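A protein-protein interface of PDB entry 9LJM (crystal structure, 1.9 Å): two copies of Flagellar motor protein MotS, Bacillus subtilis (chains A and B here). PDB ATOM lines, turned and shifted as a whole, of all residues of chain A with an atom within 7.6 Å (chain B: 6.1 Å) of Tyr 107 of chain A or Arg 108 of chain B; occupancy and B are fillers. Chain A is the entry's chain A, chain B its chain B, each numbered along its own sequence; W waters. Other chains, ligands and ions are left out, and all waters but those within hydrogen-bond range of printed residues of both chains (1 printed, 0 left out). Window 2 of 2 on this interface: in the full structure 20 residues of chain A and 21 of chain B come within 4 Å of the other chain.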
ATOM      1  N   SER A 105      22.144  24.966   8.422  1.00  0.00           N
ATOM      2  CA  SER A 105      23.573  24.755   8.243  1.00  0.00           C
ATOM      3  C   SER A 105      23.818  23.706   7.171  1.00  0.00           C
ATOM      4  O   SER A 105      24.309  22.611   7.462  1.00  0.00           O
ATOM      5  CB  SER A 105      24.227  24.334   9.562  1.00  0.00           C
ATOM      6  OG  SER A 105      25.604  24.052   9.379  1.00  0.00           O
ATOM      7  N   THR A 106      23.472  24.031   5.934  1.00  0.00           N
ATOM      8  CA  THR A 106      23.685  23.145   4.803  1.00  0.00           C
ATOM      9  C   THR A 106      24.828  23.670   3.945  1.00  0.00           C
ATOM     10  O   THR A 106      25.344  24.771   4.155  1.00  0.00           O
ATOM     11  CB  THR A 106      22.407  23.012   3.967  1.00  0.00           C
ATOM     12  OG1 THR A 106      22.127  24.258   3.319  1.00  0.00           O
ATOM     13  CG2 THR A 106      21.232  22.632   4.857  1.00  0.00           C
ATOM     14  N   TYR A 107      25.221  22.852   2.967  1.00  0.00           N
ATOM     15  CA  TYR A 107      26.249  23.268   2.018  1.00  0.00           C
ATOM     16  C   TYR A 107      25.812  24.509   1.250  1.00  0.00           C
ATOM     17  O   TYR A 107      26.614  25.422   1.014  1.00  0.00           O
ATOM     18  CB  TYR A 107      26.557  22.120   1.056  1.00  0.00           C
ATOM     19  CG  TYR A 107      27.602  22.444   0.013  1.00  0.00           C
ATOM     20  CD1 TYR A 107      28.906  22.750   0.381  1.00  0.00           C
ATOM     21  CD2 TYR A 107      27.287  22.442  -1.341  1.00  0.00           C
ATOM     22  CE1 TYR A 107      29.868  23.044  -0.567  1.00  0.00           C
ATOM     23  CE2 TYR A 107      28.242  22.737  -2.298  1.00  0.00           C
ATOM     24  CZ  TYR A 107      29.532  23.036  -1.905  1.00  0.00           C
ATOM     25  OH  TYR A 107      30.490  23.331  -2.849  1.00  0.00           O
ATOM     26  N   ARG A 108      24.536  24.566   0.867  1.00  0.00           N
ATOM     27  CA  ARG A 108      24.025  25.676   0.073  1.00  0.00           C
ATOM     28  C   ARG A 108      23.786  26.931   0.906  1.00  0.00           C
ATOM     29  O   ARG A 108      23.939  28.045   0.392  1.00  0.00           O
ATOM     30  CB  ARG A 108      22.738  25.244  -0.633  1.00  0.00           C
ATOM     31  CG  ARG A 108      22.083  26.318  -1.478  1.00  0.00           C
ATOM     32  CD  ARG A 108      22.592  26.340  -2.911  1.00  0.00           C
ATOM     33  NE  ARG A 108      21.976  27.405  -3.697  1.00  0.00           N
ATOM     34  CZ  ARG A 108      22.063  28.703  -3.430  1.00  0.00           C
ATOM     35  NH1 ARG A 108      22.792  29.161  -2.425  1.00  0.00           N
ATOM     36  NH2 ARG A 108      21.408  29.568  -4.201  1.00  0.00           N
ATOM     37  N   TYR A 109      23.428  26.782   2.181  1.00  0.00           N
ATOM     38  CA  TYR A 109      23.138  27.922   3.052  1.00  0.00           C
ATOM     39  C   TYR A 109      23.784  27.681   4.410  1.00  0.00           C
ATOM     40  O   TYR A 109      23.180  27.072   5.301  1.00  0.00           O
ATOM     41  CB  TYR A 109      21.632  28.137   3.204  1.00  0.00           C
ATOM     42  CG  TYR A 109      20.839  28.080   1.919  1.00  0.00           C
ATOM     43  CD1 TYR A 109      20.946  29.087   0.972  1.00  0.00           C
ATOM     44  CD2 TYR A 109      19.968  27.031   1.662  1.00  0.00           C
ATOM     45  CE1 TYR A 109      20.224  29.046  -0.200  1.00  0.00           C
ATOM     46  CE2 TYR A 109      19.236  26.982   0.490  1.00  0.00           C
ATOM     47  CZ  TYR A 109      19.367  27.995  -0.436  1.00  0.00           C
ATOM     48  OH  TYR A 109      18.646  27.954  -1.609  1.00  0.00           O
ATOM     49  N   PRO A 110      25.018  28.158   4.611  1.00  0.00           N
ATOM     50  CA  PRO A 110      25.755  27.804   5.839  1.00  0.00           C
ATOM     51  C   PRO A 110      25.279  28.520   7.097  1.00  0.00           C
ATOM     52  O   PRO A 110      25.767  28.185   8.182  1.00  0.00           O
ATOM     53  CB  PRO A 110      27.208  28.185   5.507  1.00  0.00           C
ATOM     54  CG  PRO A 110      27.222  28.553   4.053  1.00  0.00           C
ATOM     55  CD  PRO A 110      25.834  28.968   3.697  1.00  0.00           C
ATOM     56  N   SER A 111      24.366  29.482   7.001  1.00  0.00           N
ATOM     57  CA  SER A 111      23.775  30.081   8.193  1.00  0.00           C
ATOM     58  C   SER A 111      22.542  30.869   7.779  1.00  0.00           C
ATOM     59  O   SER A 111      22.249  31.025   6.590  1.00  0.00           O
ATOM     60  CB  SER A 111      24.755  30.988   8.939  1.00  0.00           C
ATOM     61  OG  SER A 111      24.886  32.229   8.270  1.00  0.00           O
ATOM     62  N   ALA A 118      20.204  35.154   0.526  1.00  0.00           N
ATOM     63  CA  ALA A 118      19.952  34.446  -0.723  1.00  0.00           C
ATOM     64  C   ALA A 118      18.504  34.590  -1.172  1.00  0.00           C
ATOM     65  O   ALA A 118      18.222  34.541  -2.374  1.00  0.00           O
ATOM     66  CB  ALA A 118      20.309  32.967  -0.580  1.00  0.00           C
ATOM     67  N   GLY B  67      35.336  33.223  -6.933  1.00  0.00           N
ATOM     68  CA  GLY B  67      34.003  32.686  -7.123  1.00  0.00           C
ATOM     69  C   GLY B  67      33.369  32.030  -5.918  1.00  0.00           C
ATOM     70  O   GLY B  67      32.307  31.416  -6.059  1.00  0.00           O
ATOM     71  N   GLU B  68      33.971  32.138  -4.736  1.00  0.00           N
ATOM     72  CA  GLU B  68      33.441  31.489  -3.547  1.00  0.00           C
ATOM     73  C   GLU B  68      33.137  32.514  -2.464  1.00  0.00           C
ATOM     74  O   GLU B  68      33.629  33.645  -2.488  1.00  0.00           O
ATOM     75  CB  GLU B  68      34.415  30.433  -3.011  1.00  0.00           C
ATOM     76  CG  GLU B  68      34.469  29.177  -3.861  1.00  0.00           C
ATOM     77  CD  GLU B  68      35.161  28.029  -3.160  1.00  0.00           C
ATOM     78  OE1 GLU B  68      34.604  27.514  -2.165  1.00  0.00           O
ATOM     79  OE2 GLU B  68      36.268  27.649  -3.597  1.00  0.00           O
ATOM     80  N   ALA B  69      32.310  32.096  -1.503  1.00  0.00           N
ATOM     81  CA  ALA B  69      31.923  32.940  -0.379  1.00  0.00           C
ATOM     82  C   ALA B  69      32.306  32.327   0.961  1.00  0.00           C
ATOM     83  O   ALA B  69      31.864  32.815   2.009  1.00  0.00           O
ATOM     84  CB  ALA B  69      30.418  33.226  -0.417  1.00  0.00           C
ATOM     85  N   LYS B  70      33.108  31.268   0.960  1.00  0.00           N
ATOM     86  CA  LYS B  70      33.602  30.684   2.197  1.00  0.00           C
ATOM     87  C   LYS B  70      34.851  31.438   2.635  1.00  0.00           C
ATOM     88  O   LYS B  70      35.789  31.602   1.851  1.00  0.00           O
ATOM     89  CB  LYS B  70      33.907  29.198   2.010  1.00  0.00           C
ATOM     90  CG  LYS B  70      34.199  28.466   3.305  1.00  0.00           C
ATOM     91  CD  LYS B  70      35.085  27.257   3.077  1.00  0.00           C
ATOM     92  CE  LYS B  70      36.044  27.066   4.240  1.00  0.00           C
ATOM     93  NZ  LYS B  70      37.387  27.652   3.964  1.00  0.00           N
ATOM     94  N   THR B 106      26.798  29.196 -10.756  1.00  0.00           N
ATOM     95  CA  THR B 106      27.130  27.903 -10.183  1.00  0.00           C
ATOM     96  C   THR B 106      25.967  27.394  -9.334  1.00  0.00           C
ATOM     97  O   THR B 106      24.871  27.968  -9.317  1.00  0.00           O
ATOM     98  CB  THR B 106      28.425  27.988  -9.367  1.00  0.00           C
ATOM     99  OG1 THR B 106      28.125  28.361  -8.016  1.00  0.00           O
ATOM    100  CG2 THR B 106      29.381  28.996  -9.975  1.00  0.00           C
ATOM    101  N   TYR B 107      26.207  26.296  -8.616  1.00  0.00           N
ATOM    102  CA  TYR B 107      25.167  25.695  -7.790  1.00  0.00           C
ATOM    103  C   TYR B 107      24.855  26.565  -6.578  1.00  0.00           C
ATOM    104  O   TYR B 107      23.686  26.817  -6.264  1.00  0.00           O
ATOM    105  CB  TYR B 107      25.605  24.294  -7.359  1.00  0.00           C
ATOM    106  CG  TYR B 107      24.635  23.581  -6.447  1.00  0.00           C
ATOM    107  CD1 TYR B 107      23.347  23.281  -6.868  1.00  0.00           C
ATOM    108  CD2 TYR B 107      25.013  23.195  -5.167  1.00  0.00           C
ATOM    109  CE1 TYR B 107      22.458  22.623  -6.039  1.00  0.00           C
ATOM    110  CE2 TYR B 107      24.133  22.537  -4.330  1.00  0.00           C
ATOM    111  CZ  TYR B 107      22.856  22.254  -4.770  1.00  0.00           C
ATOM    112  OH  TYR B 107      21.975  21.598  -3.941  1.00  0.00           O
ATOM    113  N   ARG B 108      25.893  27.039  -5.887  1.00  0.00           N
ATOM    114  CA  ARG B 108      25.701  27.821  -4.672  1.00  0.00           C
ATOM    115  C   ARG B 108      25.398  29.287  -4.949  1.00  0.00           C
ATOM    116  O   ARG B 108      24.814  29.954  -4.088  1.00  0.00           O
ATOM    117  CB  ARG B 108      26.938  27.707  -3.777  1.00  0.00           C
ATOM    118  CG  ARG B 108      26.805  26.667  -2.675  1.00  0.00           C
ATOM    119  CD  ARG B 108      28.137  26.379  -1.992  1.00  0.00           C
ATOM    120  NE  ARG B 108      29.261  26.448  -2.919  1.00  0.00           N
ATOM    121  CZ  ARG B 108      30.497  26.786  -2.576  1.00  0.00           C
ATOM    122  NH1 ARG B 108      30.811  27.079  -1.324  1.00  0.00           N
ATOM    123  NH2 ARG B 108      31.442  26.828  -3.511  1.00  0.00           N
ATOM    124  N   TYR B 109      25.774  29.803  -6.120  1.00  0.00           N
ATOM    125  CA  TYR B 109      25.605  31.217  -6.454  1.00  0.00           C
ATOM    126  C   TYR B 109      25.032  31.359  -7.857  1.00  0.00           C
ATOM    127  O   TYR B 109      25.775  31.409  -8.848  1.00  0.00           O
ATOM    128  CB  TYR B 109      26.922  31.976  -6.302  1.00  0.00           C
ATOM    129  CG  TYR B 109      27.728  31.537  -5.095  1.00  0.00           C
ATOM    130  CD1 TYR B 109      27.288  31.809  -3.805  1.00  0.00           C
ATOM    131  CD2 TYR B 109      28.911  30.827  -5.247  1.00  0.00           C
ATOM    132  CE1 TYR B 109      28.016  31.402  -2.698  1.00  0.00           C
ATOM    133  CE2 TYR B 109      29.642  30.413  -4.148  1.00  0.00           C
ATOM    134  CZ  TYR B 109      29.191  30.704  -2.877  1.00  0.00           C
ATOM    135  OH  TYR B 109      29.921  30.292  -1.784  1.00  0.00           O
ATOM    136  N   PRO B 110      23.702  31.437  -7.979  1.00  0.00           N
ATOM    137  CA  PRO B 110      23.080  31.565  -9.307  1.00  0.00           C
ATOM    138  C   PRO B 110      23.357  32.886 -10.018  1.00  0.00           C
ATOM    139  O   PRO B 110      23.101  32.961 -11.228  1.00  0.00           O
ATOM    140  CB  PRO B 110      21.581  31.405  -9.011  1.00  0.00           C
ATOM    141  CG  PRO B 110      21.517  30.715  -7.686  1.00  0.00           C
ATOM    142  CD  PRO B 110      22.700  31.214  -6.924  1.00  0.00           C
ATOM    143  N   GLU B 114      23.526  37.028  -5.570  1.00  0.00           N
ATOM    144  CA  GLU B 114      23.687  35.969  -4.579  1.00  0.00           C
ATOM    145  C   GLU B 114      25.123  35.902  -4.070  1.00  0.00           C
ATOM    146  O   GLU B 114      25.364  35.782  -2.862  1.00  0.00           O
ATOM    147  CB  GLU B 114      23.281  34.630  -5.194  1.00  0.00           C
ATOM    148  CG  GLU B 114      23.822  33.416  -4.459  1.00  0.00           C
ATOM    149  CD  GLU B 114      22.911  32.937  -3.354  1.00  0.00           C
ATOM    150  OE1 GLU B 114      21.914  32.246  -3.667  1.00  0.00           O
ATOM    151  OE2 GLU B 114      23.182  33.247  -2.180  1.00  0.00           O
ATOM    152  N   ALA B 118      26.198  36.561  -0.299  1.00  0.00           N
ATOM    153  CA  ALA B 118      26.768  35.460   0.470  1.00  0.00           C
ATOM    154  C   ALA B 118      28.130  35.825   1.042  1.00  0.00           C
ATOM    155  O   ALA B 118      28.503  35.342   2.118  1.00  0.00           O
ATOM    156  CB  ALA B 118      26.878  34.209  -0.401  1.00  0.00           C
HETATM  157  O   HOH W   1      19.281  33.033  -4.575  1.00  0.00           O
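OH of Tyr 107 of chain A sits at hydrogen-bond distance from NE of Arg 108 of chain B, at 3.4 Å.
NE of Arg 108 of chain A is in hydrogen-bond range of O of Tyr 107 of chain B (3.1 Å).
NH1 of Arg 108 of chain A is in hydrogen-bond range of O of Arg 108 of chain B (2.7 Å).
NH2 of Arg 108 of chain A is in salt-bridge range of OE1 of Glu 114 of chain B, 2.8 Å away.
OG1 of Thr 106 of chain A sits close to N of Arg 108 of chain A, 3.5 Å away.
The guanidinium group (NH2) of Arg 108 of chain B is in salt-bridge range of the side-chain carboxylate (OE1) of Glu 68 of chain B, at 3.5 Å.
OG1 of Thr 106 of chain B is in hydrogen-bond range of N of Arg 108 of chain B, at 3.4 Å.
The side-chain hydroxyl (OH) of Tyr 109 of chain B lies within hydrogen-bond range of the guanidinium group (NH1) of Arg 108 of chain B (3.4 Å).
Among the printed residues, merely in contact across the chains: Arg 108 of chain A with Pro 110 of chain B and Ala 118 of chain A with Glu 114 of chain B.
Printed residues of chain A within 4 Å of Tyr 107 of chain B: Arg 108 (3.1 Å).
Of the printed residues of chain A, Glu 114 of chain B touches Arg 108 and Ala 118.
Ala 118 of chain B touches none of the printed residues of chain A.
The nearest printed residue of chain A that does not touch Arg 108 of chain B is Tyr 109 of chain A (5.9 Å).
Hydrophobic or aromatic side chains of chain A that line the printed part of chain B: Tyr 107 and Ala 118.
Printed residues of chain B that touch a printed residue of chain A: Tyr 107, Arg 108, Pro 110 and Glu 114.
Among the printed residues, 6 pairs touch across the chains.
Among the printed residues, Asp or Glu carboxylates within 4 Å of a Lys or Arg side-chain nitrogen of the other chain: Arg 108 of chain A with Glu 114 of chain B (2.8 Å).
Tyr 107 of chain A touches Arg 108 of chain B, and with the chains exchanged Arg 108 of chain A touches Tyr 107 of chain B.
Arg 108 of chain B touches its own counterpart, Arg 108 of chain A.
Arg 108 of chain A touches Pro 110 of chain B, but with the chains exchanged Pro 110 of chain A does not touch Arg 108 of chain B (6.5 Å).
Water W1 bridges the backbone carbonyl oxygen (O) of Ala 118 of chain A (2.9 Å) and the side-chain carboxylate (OE1) of Glu 114 of chain B (2.9 Å).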
